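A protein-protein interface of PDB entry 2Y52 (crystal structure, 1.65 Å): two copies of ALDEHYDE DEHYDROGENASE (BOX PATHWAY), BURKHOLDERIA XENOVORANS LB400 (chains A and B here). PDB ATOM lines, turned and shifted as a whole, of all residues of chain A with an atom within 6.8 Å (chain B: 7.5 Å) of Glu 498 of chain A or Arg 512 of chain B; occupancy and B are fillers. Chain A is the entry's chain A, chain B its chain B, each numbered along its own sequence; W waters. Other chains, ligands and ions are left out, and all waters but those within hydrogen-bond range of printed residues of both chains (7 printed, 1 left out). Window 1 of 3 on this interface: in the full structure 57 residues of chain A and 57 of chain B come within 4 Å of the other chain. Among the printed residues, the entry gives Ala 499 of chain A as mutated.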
ATOM      1  N   ASN A 258      26.056  32.742  19.355  1.00  0.00           N
ATOM      2  CA  ASN A 258      25.723  31.673  20.321  1.00  0.00           C
ATOM      3  C   ASN A 258      25.635  32.291  21.694  1.00  0.00           C
ATOM      4  O   ASN A 258      26.552  32.988  22.109  1.00  0.00           O
ATOM      5  CB  ASN A 258      26.851  30.614  20.373  1.00  0.00           C
ATOM      6  CG  ASN A 258      26.400  29.261  20.967  1.00  0.00           C
ATOM      7  OD1 ASN A 258      26.762  28.858  22.131  1.00  0.00           O
ATOM      8  ND2 ASN A 258      25.663  28.531  20.158  1.00  0.00           N
ATOM      9  N   VAL A 259      24.563  31.916  22.416  1.00  0.00           N
ATOM     10  CA  VAL A 259      24.289  32.347  23.741  1.00  0.00           C
ATOM     11  C   VAL A 259      24.229  31.103  24.704  1.00  0.00           C
ATOM     12  O   VAL A 259      23.587  30.065  24.399  1.00  0.00           O
ATOM     13  CB  VAL A 259      22.950  33.188  23.794  1.00  0.00           C
ATOM     14  CG1 VAL A 259      22.418  33.356  25.242  1.00  0.00           C
ATOM     15  CG2 VAL A 259      23.126  34.597  23.079  1.00  0.00           C
ATOM     16  N   GLU A 260      24.967  31.242  25.798  1.00  0.00           N
ATOM     17  CA  GLU A 260      24.895  30.383  27.019  1.00  0.00           C
ATOM     18  C   GLU A 260      24.466  31.237  28.173  1.00  0.00           C
ATOM     19  O   GLU A 260      25.156  32.209  28.504  1.00  0.00           O
ATOM     20  CB  GLU A 260      26.292  29.779  27.324  1.00  0.00           C
ATOM     21  CG  GLU A 260      26.646  28.737  26.279  1.00  0.00           C
ATOM     22  CD  GLU A 260      28.103  28.311  26.272  1.00  0.00           C
ATOM     23  OE1 GLU A 260      28.899  28.873  27.084  1.00  0.00           O
ATOM     24  OE2 GLU A 260      28.395  27.423  25.405  1.00  0.00           O
ATOM     25  N   ALA A 459      15.111  14.612  26.320  1.00  0.00           N
ATOM     26  CA  ALA A 459      16.018  15.075  25.271  1.00  0.00           C
ATOM     27  C   ALA A 459      15.561  16.407  24.568  1.00  0.00           C
ATOM     28  O   ALA A 459      16.421  17.189  24.098  1.00  0.00           O
ATOM     29  CB  ALA A 459      16.299  13.920  24.214  1.00  0.00           C
ATOM     30  N   ASP A 460      14.245  16.668  24.492  1.00  0.00           N
ATOM     31  CA  ASP A 460      13.774  17.833  23.717  1.00  0.00           C
ATOM     32  C   ASP A 460      13.860  19.106  24.534  1.00  0.00           C
ATOM     33  O   ASP A 460      13.616  20.201  24.004  1.00  0.00           O
ATOM     34  CB  ASP A 460      12.373  17.663  23.106  1.00  0.00           C
ATOM     35  CG  ASP A 460      11.267  17.462  24.152  1.00  0.00           C
ATOM     36  OD1 ASP A 460      11.441  17.869  25.322  1.00  0.00           O
ATOM     37  OD2 ASP A 460      10.157  16.966  23.758  1.00  0.00           O
ATOM     38  N   HIS A 462      16.662  19.438  27.006  1.00  0.00           N
ATOM     39  CA  HIS A 462      17.987  19.467  27.638  1.00  0.00           C
ATOM     40  C   HIS A 462      19.024  19.172  26.589  1.00  0.00           C
ATOM     41  O   HIS A 462      18.898  18.146  25.861  1.00  0.00           O
ATOM     42  CB  HIS A 462      18.086  18.370  28.767  1.00  0.00           C
ATOM     43  CG  HIS A 462      17.139  18.630  29.927  1.00  0.00           C
ATOM     44  ND1 HIS A 462      15.806  18.258  29.883  1.00  0.00           N
ATOM     45  CD2 HIS A 462      17.312  19.297  31.111  1.00  0.00           C
ATOM     46  CE1 HIS A 462      15.189  18.734  30.963  1.00  0.00           C
ATOM     47  NE2 HIS A 462      16.091  19.285  31.762  1.00  0.00           N
ATOM     48  N   GLY A 463      20.079  20.004  26.541  1.00  0.00           N
ATOM     49  CA  GLY A 463      21.156  19.788  25.540  1.00  0.00           C
ATOM     50  C   GLY A 463      21.957  18.513  25.829  1.00  0.00           C
ATOM     51  O   GLY A 463      22.669  18.050  24.969  1.00  0.00           O
ATOM     52  N   ARG A 464      21.896  18.022  27.069  1.00  0.00           N
ATOM     53  CA  ARG A 464      22.621  16.822  27.521  1.00  0.00           C
ATOM     54  C   ARG A 464      21.822  16.119  28.589  1.00  0.00           C
ATOM     55  O   ARG A 464      21.299  16.698  29.476  1.00  0.00           O
ATOM     56  CB  ARG A 464      24.058  17.101  28.045  1.00  0.00           C
ATOM     57  CG  ARG A 464      24.930  15.876  28.404  1.00  0.00           C
ATOM     58  CD  ARG A 464      26.421  16.180  28.467  1.00  0.00           C
ATOM     59  NE  ARG A 464      26.709  17.377  29.284  1.00  0.00           N
ATOM     60  CZ  ARG A 464      26.894  17.342  30.598  1.00  0.00           C
ATOM     61  NH1 ARG A 464      26.914  16.189  31.270  1.00  0.00           N
ATOM     62  NH2 ARG A 464      26.993  18.489  31.299  1.00  0.00           N
ATOM     63  N   LEU A 487      27.901  17.305  22.899  1.00  0.00           N
ATOM     64  CA  LEU A 487      27.211  18.655  22.817  1.00  0.00           C
ATOM     65  C   LEU A 487      27.161  19.449  24.144  1.00  0.00           C
ATOM     66  O   LEU A 487      26.801  18.870  25.182  1.00  0.00           O
ATOM     67  CB  LEU A 487      25.788  18.569  22.146  1.00  0.00           C
ATOM     68  CG  LEU A 487      24.959  19.919  22.057  1.00  0.00           C
ATOM     69  CD1 LEU A 487      25.516  20.754  20.929  1.00  0.00           C
ATOM     70  CD2 LEU A 487      23.599  19.529  21.686  1.00  0.00           C
ATOM     71  N   HIS A 488      27.547  20.743  24.093  1.00  0.00           N
ATOM     72  CA  HIS A 488      27.318  21.665  25.255  1.00  0.00           C
ATOM     73  C   HIS A 488      26.382  22.828  24.908  1.00  0.00           C
ATOM     74  O   HIS A 488      26.664  23.584  23.938  1.00  0.00           O
ATOM     75  CB  HIS A 488      28.645  22.248  25.789  1.00  0.00           C
ATOM     76  CG  HIS A 488      28.480  23.202  26.951  1.00  0.00           C
ATOM     77  ND1 HIS A 488      28.090  22.770  28.217  1.00  0.00           N
ATOM     78  CD2 HIS A 488      28.683  24.552  27.059  1.00  0.00           C
ATOM     79  CE1 HIS A 488      28.039  23.808  29.036  1.00  0.00           C
ATOM     80  NE2 HIS A 488      28.417  24.890  28.362  1.00  0.00           N
ATOM     81  N   GLY A 489      25.286  22.980  25.648  1.00  0.00           N
ATOM     82  CA  GLY A 489      24.315  24.089  25.312  1.00  0.00           C
ATOM     83  C   GLY A 489      22.929  23.579  25.710  1.00  0.00           C
ATOM     84  O   GLY A 489      22.809  22.412  26.159  1.00  0.00           O
ATOM     85  N   GLY A 490      21.915  24.424  25.554  1.00  0.00           N
ATOM     86  CA  GLY A 490      20.551  23.965  25.787  1.00  0.00           C
ATOM     87  C   GLY A 490      19.532  24.929  25.247  1.00  0.00           C
ATOM     88  O   GLY A 490      19.854  26.073  25.001  1.00  0.00           O
ATOM     89  N   PRO A 491      18.288  24.466  25.104  1.00  0.00           N
ATOM     90  CA  PRO A 491      17.257  25.260  24.481  1.00  0.00           C
ATOM     91  C   PRO A 491      16.612  26.243  25.459  1.00  0.00           C
ATOM     92  O   PRO A 491      16.900  26.244  26.705  1.00  0.00           O
ATOM     93  CB  PRO A 491      16.241  24.210  23.986  1.00  0.00           C
ATOM     94  CG  PRO A 491      16.460  22.987  25.009  1.00  0.00           C
ATOM     95  CD  PRO A 491      17.937  23.016  25.242  1.00  0.00           C
ATOM     96  N   GLY A 496      19.624  28.534  23.813  1.00  0.00           N
ATOM     97  CA  GLY A 496      19.445  28.174  22.472  1.00  0.00           C
ATOM     98  C   GLY A 496      20.777  27.893  21.728  1.00  0.00           C
ATOM     99  O   GLY A 496      20.772  27.732  20.511  1.00  0.00           O
ATOM    100  N   GLY A 497      21.876  27.761  22.459  1.00  0.00           N
ATOM    101  CA  GLY A 497      23.221  27.634  21.839  1.00  0.00           C
ATOM    102  C   GLY A 497      23.652  26.168  21.747  1.00  0.00           C
ATOM    103  O   GLY A 497      23.037  25.245  22.371  1.00  0.00           O
ATOM    104  N   GLU A 498      24.706  25.957  20.945  1.00  0.00           N
ATOM    105  CA  GLU A 498      25.389  24.663  20.721  1.00  0.00           C
ATOM    106  C   GLU A 498      26.855  24.956  20.561  1.00  0.00           C
ATOM    107  O   GLU A 498      27.263  25.798  19.716  1.00  0.00           O
ATOM    108  CB  GLU A 498      24.846  23.912  19.474  1.00  0.00           C
ATOM    109  CG  GLU A 498      23.342  23.598  19.573  1.00  0.00           C
ATOM    110  CD  GLU A 498      22.839  22.521  18.591  1.00  0.00           C
ATOM    111  OE1 GLU A 498      23.648  21.887  17.863  1.00  0.00           O
ATOM    112  OE2 GLU A 498      21.589  22.334  18.548  1.00  0.00           O
ATOM    113  N   ALA A 499      27.652  24.230  21.336  1.00  0.00           N
ATOM    114  CA  ALA A 499      29.119  24.239  21.257  1.00  0.00           C
ATOM    115  C   ALA A 499      29.680  22.838  21.476  1.00  0.00           C
ATOM    116  O   ALA A 499      28.967  21.894  21.847  1.00  0.00           O
ATOM    117  CB  ALA A 499      29.619  25.158  22.349  1.00  0.00           C
ATOM    118  N   LEU A 500      30.977  22.671  21.256  1.00  0.00           N
ATOM    119  CA  LEU A 500      31.587  21.344  21.443  1.00  0.00           C
ATOM    120  C   LEU A 500      30.886  20.263  20.563  1.00  0.00           C
ATOM    121  O   LEU A 500      30.564  20.521  19.364  1.00  0.00           O
ATOM    122  CB  LEU A 500      31.784  20.968  22.946  1.00  0.00           C
ATOM    123  CG  LEU A 500      32.700  21.919  23.703  1.00  0.00           C
ATOM    124  CD1 LEU A 500      32.728  21.677  25.170  1.00  0.00           C
ATOM    125  CD2 LEU A 500      34.167  21.902  23.241  1.00  0.00           C
ATOM    126  N   ARG A 504      31.321  18.683  15.526  1.00  0.00           N
ATOM    127  CA  ARG A 504      30.103  19.449  15.335  1.00  0.00           C
ATOM    128  C   ARG A 504      30.417  20.919  15.578  1.00  0.00           C
ATOM    129  O   ARG A 504      29.869  21.772  14.926  1.00  0.00           O
ATOM    130  CB  ARG A 504      28.970  18.963  16.275  1.00  0.00           C
ATOM    131  CG  ARG A 504      28.478  17.502  15.900  1.00  0.00           C
ATOM    132  CD  ARG A 504      27.455  17.038  16.956  1.00  0.00           C
ATOM    133  NE  ARG A 504      26.995  15.643  16.721  1.00  0.00           N
ATOM    134  CZ  ARG A 504      27.699  14.580  17.077  1.00  0.00           C
ATOM    135  NH1 ARG A 504      28.899  14.666  17.655  1.00  0.00           N
ATOM    136  NH2 ARG A 504      27.189  13.385  16.814  1.00  0.00           N
ATOM    137  N   ALA A 505      31.427  21.149  16.404  1.00  0.00           N
ATOM    138  CA  ALA A 505      31.779  22.536  16.835  1.00  0.00           C
ATOM    139  C   ALA A 505      32.324  23.325  15.654  1.00  0.00           C
ATOM    140  O   ALA A 505      32.319  24.580  15.655  1.00  0.00           O
ATOM    141  CB  ALA A 505      32.842  22.497  17.942  1.00  0.00           C
ATOM    142  N   PHE A 508      30.015  26.016  13.363  1.00  0.00           N
ATOM    143  CA  PHE A 508      29.798  27.449  13.809  1.00  0.00           C
ATOM    144  C   PHE A 508      30.848  28.371  13.191  1.00  0.00           C
ATOM    145  O   PHE A 508      30.543  29.578  12.985  1.00  0.00           O
ATOM    146  CB  PHE A 508      29.897  27.480  15.350  1.00  0.00           C
ATOM    147  CG  PHE A 508      29.559  28.815  15.991  1.00  0.00           C
ATOM    148  CD1 PHE A 508      28.230  29.254  16.040  1.00  0.00           C
ATOM    149  CD2 PHE A 508      30.573  29.630  16.513  1.00  0.00           C
ATOM    150  CE1 PHE A 508      27.949  30.440  16.631  1.00  0.00           C
ATOM    151  CE2 PHE A 508      30.240  30.828  17.177  1.00  0.00           C
ATOM    152  CZ  PHE A 508      28.971  31.205  17.195  1.00  0.00           C
ATOM    153  N   ASP B 130      21.907  11.189  15.653  1.00  0.00           N
ATOM    154  CA  ASP B 130      22.895  12.075  15.067  1.00  0.00           C
ATOM    155  C   ASP B 130      24.267  11.489  15.230  1.00  0.00           C
ATOM    156  O   ASP B 130      24.840  11.588  16.326  1.00  0.00           O
ATOM    157  CB  ASP B 130      22.863  13.385  15.835  1.00  0.00           C
ATOM    158  CG  ASP B 130      23.898  14.433  15.302  1.00  0.00           C
ATOM    159  OD1 ASP B 130      24.800  14.119  14.553  1.00  0.00           O
ATOM    160  OD2 ASP B 130      23.761  15.623  15.586  1.00  0.00           O
ATOM    161  N   HIS B 146      24.361  11.048  20.313  1.00  0.00           N
ATOM    162  CA  HIS B 146      23.492  12.257  20.117  1.00  0.00           C
ATOM    163  C   HIS B 146      22.200  11.891  19.423  1.00  0.00           C
ATOM    164  O   HIS B 146      22.162  10.924  18.597  1.00  0.00           O
ATOM    165  CB  HIS B 146      24.235  13.343  19.324  1.00  0.00           C
ATOM    166  CG  HIS B 146      25.411  13.904  20.050  1.00  0.00           C
ATOM    167  ND1 HIS B 146      26.628  13.239  20.139  1.00  0.00           N
ATOM    168  CD2 HIS B 146      25.589  15.090  20.669  1.00  0.00           C
ATOM    169  CE1 HIS B 146      27.475  13.976  20.841  1.00  0.00           C
ATOM    170  NE2 HIS B 146      26.864  15.112  21.161  1.00  0.00           N
ATOM    171  N   VAL B 147      21.127  12.631  19.774  1.00  0.00           N
ATOM    172  CA  VAL B 147      19.863  12.388  19.177  1.00  0.00           C
ATOM    173  C   VAL B 147      19.190  13.692  18.798  1.00  0.00           C
ATOM    174  O   VAL B 147      19.498  14.771  19.352  1.00  0.00           O
ATOM    175  CB  VAL B 147      18.882  11.609  20.151  1.00  0.00           C
ATOM    176  CG1 VAL B 147      19.389  10.232  20.401  1.00  0.00           C
ATOM    177  CG2 VAL B 147      18.647  12.363  21.455  1.00  0.00           C
ATOM    178  N   LEU B 148      18.240  13.557  17.872  1.00  0.00           N
ATOM    179  CA  LEU B 148      17.405  14.667  17.404  1.00  0.00           C
ATOM    180  C   LEU B 148      15.924  14.414  17.789  1.00  0.00           C
ATOM    181  O   LEU B 148      15.358  13.372  17.401  1.00  0.00           O
ATOM    182  CB  LEU B 148      17.523  14.840  15.892  1.00  0.00           C
ATOM    183  CG  LEU B 148      18.822  15.385  15.284  1.00  0.00           C
ATOM    184  CD1 LEU B 148      18.769  15.315  13.775  1.00  0.00           C
ATOM    185  CD2 LEU B 148      19.197  16.748  15.748  1.00  0.00           C
ATOM    186  N   SER B 149      15.264  15.376  18.430  1.00  0.00           N
ATOM    187  CA  SER B 149      13.845  15.224  18.881  1.00  0.00           C
ATOM    188  C   SER B 149      13.026  16.409  18.371  1.00  0.00           C
ATOM    189  O   SER B 149      13.574  17.521  18.387  1.00  0.00           O
ATOM    190  CB  SER B 149      13.735  15.188  20.430  1.00  0.00           C
ATOM    191  OG  SER B 149      14.607  14.207  21.046  1.00  0.00           O
ATOM    192  N   ARG B 256      14.245  30.181  17.309  1.00  0.00           N
ATOM    193  CA  ARG B 256      15.112  30.079  16.105  1.00  0.00           C
ATOM    194  C   ARG B 256      14.496  30.771  14.931  1.00  0.00           C
ATOM    195  O   ARG B 256      13.294  30.661  14.685  1.00  0.00           O
ATOM    196  CB  ARG B 256      15.259  28.635  15.628  1.00  0.00           C
ATOM    197  CG  ARG B 256      15.838  27.697  16.496  1.00  0.00           C
ATOM    198  CD  ARG B 256      16.473  26.605  15.590  1.00  0.00           C
ATOM    199  NE  ARG B 256      17.238  25.808  16.528  1.00  0.00           N
ATOM    200  CZ  ARG B 256      17.102  24.490  16.669  1.00  0.00           C
ATOM    201  NH1 ARG B 256      16.188  23.823  15.973  1.00  0.00           N
ATOM    202  NH2 ARG B 256      17.871  23.901  17.570  1.00  0.00           N
ATOM    203  N   ARG B 504      19.489  17.512   5.697  1.00  0.00           N
ATOM    204  CA  ARG B 504      19.978  18.685   6.443  1.00  0.00           C
ATOM    205  C   ARG B 504      18.872  19.570   6.977  1.00  0.00           C
ATOM    206  O   ARG B 504      18.971  20.196   8.093  1.00  0.00           O
ATOM    207  CB  ARG B 504      20.957  19.485   5.555  1.00  0.00           C
ATOM    208  CG  ARG B 504      22.222  18.587   5.177  1.00  0.00           C
ATOM    209  CD  ARG B 504      23.132  19.410   4.287  1.00  0.00           C
ATOM    210  NE  ARG B 504      24.291  18.592   3.829  1.00  0.00           N
ATOM    211  CZ  ARG B 504      24.197  17.643   2.902  1.00  0.00           C
ATOM    212  NH1 ARG B 504      23.033  17.380   2.300  1.00  0.00           N
ATOM    213  NH2 ARG B 504      25.289  16.985   2.571  1.00  0.00           N
ATOM    214  N   LEU B 506      16.110  18.819   8.294  1.00  0.00           N
ATOM    215  CA  LEU B 506      15.392  18.327   9.500  1.00  0.00           C
ATOM    216  C   LEU B 506      15.908  18.965  10.751  1.00  0.00           C
ATOM    217  O   LEU B 506      15.127  19.219  11.680  1.00  0.00           O
ATOM    218  CB  LEU B 506      15.527  16.843   9.624  1.00  0.00           C
ATOM    219  CG  LEU B 506      15.056  15.995   8.462  1.00  0.00           C
ATOM    220  CD1 LEU B 506      15.193  14.476   8.833  1.00  0.00           C
ATOM    221  CD2 LEU B 506      13.637  16.280   8.126  1.00  0.00           C
ATOM    222  N   ALA B 507      17.191  19.305  10.797  1.00  0.00           N
ATOM    223  CA  ALA B 507      17.742  19.855  12.031  1.00  0.00           C
ATOM    224  C   ALA B 507      17.084  21.152  12.496  1.00  0.00           C
ATOM    225  O   ALA B 507      16.899  21.288  13.661  1.00  0.00           O
ATOM    226  CB  ALA B 507      19.337  20.026  11.923  1.00  0.00           C
ATOM    227  N   PHE B 508      16.755  22.092  11.624  1.00  0.00           N
ATOM    228  CA  PHE B 508      16.096  23.368  12.028  1.00  0.00           C
ATOM    229  C   PHE B 508      14.835  23.081  12.848  1.00  0.00           C
ATOM    230  O   PHE B 508      14.457  23.870  13.669  1.00  0.00           O
ATOM    231  CB  PHE B 508      15.711  24.103  10.731  1.00  0.00           C
ATOM    232  CG  PHE B 508      15.128  25.481  10.925  1.00  0.00           C
ATOM    233  CD1 PHE B 508      15.944  26.493  11.358  1.00  0.00           C
ATOM    234  CD2 PHE B 508      13.778  25.740  10.622  1.00  0.00           C
ATOM    235  CE1 PHE B 508      15.409  27.763  11.535  1.00  0.00           C
ATOM    236  CE2 PHE B 508      13.261  27.004  10.818  1.00  0.00           C
ATOM    237  CZ  PHE B 508      14.111  28.010  11.233  1.00  0.00           C
ATOM    238  N   HIS B 510      14.320  20.274  14.875  1.00  0.00           N
ATOM    239  CA  HIS B 510      14.573  19.373  15.978  1.00  0.00           C
ATOM    240  C   HIS B 510      15.445  20.037  17.066  1.00  0.00           C
ATOM    241  O   HIS B 510      16.104  21.085  16.803  1.00  0.00           O
ATOM    242  CB  HIS B 510      15.274  18.080  15.449  1.00  0.00           C
ATOM    243  CG  HIS B 510      14.405  17.101  14.730  1.00  0.00           C
ATOM    244  ND1 HIS B 510      14.001  17.249  13.419  1.00  0.00           N
ATOM    245  CD2 HIS B 510      13.882  15.932  15.163  1.00  0.00           C
ATOM    246  CE1 HIS B 510      13.264  16.201  13.074  1.00  0.00           C
ATOM    247  NE2 HIS B 510      13.208  15.364  14.101  1.00  0.00           N
ATOM    248  N   ARG B 511      15.453  19.461  18.251  1.00  0.00           N
ATOM    249  CA  ARG B 511      16.389  19.823  19.301  1.00  0.00           C
ATOM    250  C   ARG B 511      17.398  18.679  19.397  1.00  0.00           C
ATOM    251  O   ARG B 511      17.021  17.537  19.449  1.00  0.00           O
ATOM    252  CB  ARG B 511      15.660  19.995  20.630  1.00  0.00           C
ATOM    253  CG  ARG B 511      14.322  20.595  20.519  1.00  0.00           C
ATOM    254  CD  ARG B 511      14.148  22.075  20.899  1.00  0.00           C
ATOM    255  NE  ARG B 511      15.224  23.000  20.600  1.00  0.00           N
ATOM    256  CZ  ARG B 511      15.010  24.243  20.166  1.00  0.00           C
ATOM    257  NH1 ARG B 511      13.807  24.609  19.757  1.00  0.00           N
ATOM    258  NH2 ARG B 511      16.027  25.058  19.976  1.00  0.00           N
ATOM    259  N   ARG B 512      18.667  19.041  19.368  1.00  0.00           N
ATOM    260  CA  ARG B 512      19.810  18.106  19.484  1.00  0.00           C
ATOM    261  C   ARG B 512      20.236  17.911  20.940  1.00  0.00           C
ATOM    262  O   ARG B 512      20.282  18.895  21.721  1.00  0.00           O
ATOM    263  CB  ARG B 512      21.017  18.607  18.628  1.00  0.00           C
ATOM    264  CG  ARG B 512      22.220  17.622  18.577  1.00  0.00           C
ATOM    265  CD  ARG B 512      23.365  18.242  17.727  1.00  0.00           C
ATOM    266  NE  ARG B 512      23.030  18.141  16.325  1.00  0.00           N
ATOM    267  CZ  ARG B 512      22.626  19.136  15.573  1.00  0.00           C
ATOM    268  NH1 ARG B 512      22.476  20.356  16.065  1.00  0.00           N
ATOM    269  NH2 ARG B 512      22.345  18.898  14.319  1.00  0.00           N
ATOM    270  N   SER B 513      20.482  16.661  21.334  1.00  0.00           N
ATOM    271  CA  SER B 513      20.916  16.328  22.707  1.00  0.00           C
ATOM    272  C   SER B 513      21.965  15.270  22.755  1.00  0.00           C
ATOM    273  O   SER B 513      21.850  14.246  22.045  1.00  0.00           O
ATOM    274  CB  SER B 513      19.694  15.937  23.530  1.00  0.00           C
ATOM    275  OG  SER B 513      19.917  15.970  24.932  1.00  0.00           O
ATOM    276  N   ALA B 514      22.945  15.481  23.625  1.00  0.00           N
ATOM    277  CA  ALA B 514      23.971  14.430  23.909  1.00  0.00           C
ATOM    278  C   ALA B 514      23.447  13.542  25.042  1.00  0.00           C
ATOM    279  O   ALA B 514      23.226  14.022  26.142  1.00  0.00           O
ATOM    280  CB  ALA B 514      25.289  15.049  24.349  1.00  0.00           C
ATOM    281  N   ILE B 515      23.222  12.262  24.750  1.00  0.00           N
ATOM    282  CA  ILE B 515      22.870  11.327  25.852  1.00  0.00           C
ATOM    283  C   ILE B 515      24.096  10.568  26.272  1.00  0.00           C
ATOM    284  O   ILE B 515      24.753   9.949  25.416  1.00  0.00           O
ATOM    285  CB  ILE B 515      21.809  10.247  25.433  1.00  0.00           C
ATOM    286  CG1 ILE B 515      20.588  10.888  24.735  1.00  0.00           C
ATOM    287  CG2 ILE B 515      21.296   9.495  26.687  1.00  0.00           C
ATOM    288  CD1 ILE B 515      19.897  12.019  25.472  1.00  0.00           C
HETATM  289  O   HOH W   1      18.479  27.853  18.811  1.00  0.00           O
HETATM  290  O   HOH W   2      20.582  21.823  21.273  1.00  0.00           O
HETATM  291  O   HOH W   3      26.512  10.586  18.378  1.00  0.00           O
HETATM  292  O   HOH W   4      19.098  21.508  18.027  1.00  0.00           O
HETATM  293  O   HOH W   5      18.698  25.139  20.880  1.00  0.00           O
HETATM  294  O   HOH W   6      20.334  24.875  18.566  1.00  0.00           O
HETATM  295  O   HOH W   7      16.914  15.833  21.505  1.00  0.00           O
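Water W7 lies within hydrogen-bond range of the backbone carbonyl oxygen of Arg 511 of chain B (2.7 Å), the side-chain hydroxyl of Ser 149 of chain B (2.9 Å) and the backbone carbonyl oxygen of Ala 459 of chain A (3.0 Å).
Water W3 lies within hydrogen-bond range of the backbone carbonyl oxygen of Asp 130 of chain B, the backbone NH of His 146 of chain B and the guanidinium group of Arg 504 of chain A.
Water W1 bridges the backbone carbonyl oxygen of Gly 496 of chain A (2.9 Å) and the guanidinium group of Arg 256 of chain B (3.3 Å).
Water W2 bridges OE2 of Glu 498 of chain A (2.9 Å) and O of Arg 512 of chain B (3.0 Å).
The backbone carbonyl oxygen (O) of Ser 149 of chain B is in hydrogen-bond range of the backbone NH (N) of Arg 511 of chain B, at 2.7 Å.
The backbone carbonyl oxygen (O) of Ser 513 of chain B sits at hydrogen-bond distance from the backbone NH (N) of Val 147 of chain B, at 2.9 Å.
ND2 of Asn 258 of chain A sits close to N of Glu 498 of chain A (2.9 Å).
N of Asp 130 of chain B sits at hydrogen-bond distance from O of His 146 of chain B, at 3.0 Å.
The guanidinium group (NE) of Arg 512 of chain B lies within salt-bridge range of the side-chain carboxylate (OD2) of Asp 130 of chain B (2.7 Å).
The backbone carbonyl oxygen (O) of His 462 of chain A sits at hydrogen-bond distance from the side-chain hydroxyl (OG) of Ser 513 of chain B, 2.6 Å away.
The backbone NH (N) of Leu 487 of chain A lies within hydrogen-bond range of a ring nitrogen (NE2) of His 146 of chain B (3.0 Å).
OE1 of Glu 498 of chain A is in salt-bridge range of NH1 of Arg 512 of chain B (2.6 Å).
A ring nitrogen (ND1) of His 146 of chain B is in hydrogen-bond range of the guanidinium group (NH2) of Arg 504 of chain A (3.4 Å).
The backbone carbonyl oxygen (O) of Gly 463 of chain A is in hydrogen-bond range of the backbone NH (N) of Ala 514 of chain B (2.9 Å).
The backbone carbonyl oxygen (O) of Gly 463 of chain A lies close to the side-chain hydroxyl (OG) of Ser 513 of chain B (3.4 Å).
The guanidinium group (NH2) of Arg 504 of chain A is in salt-bridge range of the side-chain carboxylate (OD1) of Asp 130 of chain B.
Of the 16 printed residues of chain B, 8 touch a printed residue of chain A.
Among the printed residues, Asp or Glu carboxylates within 4 Å of a Lys or Arg side-chain nitrogen of the other chain: Glu 498 of chain A with Arg 512 of chain B (2.6 Å) and Arg 504 of chain A with Asp 130 of chain B (3.4 Å).
Among the printed residues, pairs that only touch across the chains: Arg 464 of chain A with Ala 514 of chain B (3.2 Å), Leu 487 of chain A with Arg 512 of chain B (3.4 Å), Ala 459 of chain A with Ser 513 of chain B (3.6 Å), Arg 464 of chain A with Ser 513 of chain B (3.6 Å), Asp 460 of chain A with Arg 511 of chain B (3.6 Å), Ala 459 of chain A with Ser 149 of chain B (3.6 Å), Pro 491 of chain A with Arg 511 of chain B (3.7 Å), Leu 487 of chain A with Ala 514 of chain B (3.7 Å), Asp 460 of chain A with Ser 149 of chain B (3.9 Å) and Ala 459 of chain A with Val 147 of chain B (3.9 Å).
2 positions are printed for both chains.
Of the 17 pairs that touch across the chains among the printed residues, none has its exchanged pair printed and touching as well.
Printed residues of chain B within 4 Å of Glu 498 of chain A: Arg 512 (2.6 Å).
Of the printed residues of chain A, Arg 512 of chain B touches Leu 487 and Glu 498.
Printed residues of chain A within 4 Å of His 146 of chain B: Leu 487 and Arg 504.
Of the printed residues of chain A, Ser 149 of chain B touches Ala 459 and Asp 460.
Of the printed residues of chain A, Asp 130 of chain B touches Arg 504.
Of the printed residues of chain B, Arg 464 of chain A touches Ser 513 (3.6 Å) and Ala 514 (3.2 Å).
Phe 508 of chain A touches none of the printed residues of chain B.
Arg 256 of chain B touches none of the printed residues of chain A.
The nearest residue of chain B that does not touch Glu 498 of chain A is Arg 256 of chain B (4.2 Å).
The nearest printed residue of chain A that does not touch Arg 512 of chain B is Gly 463 of chain A (4.02 Å).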
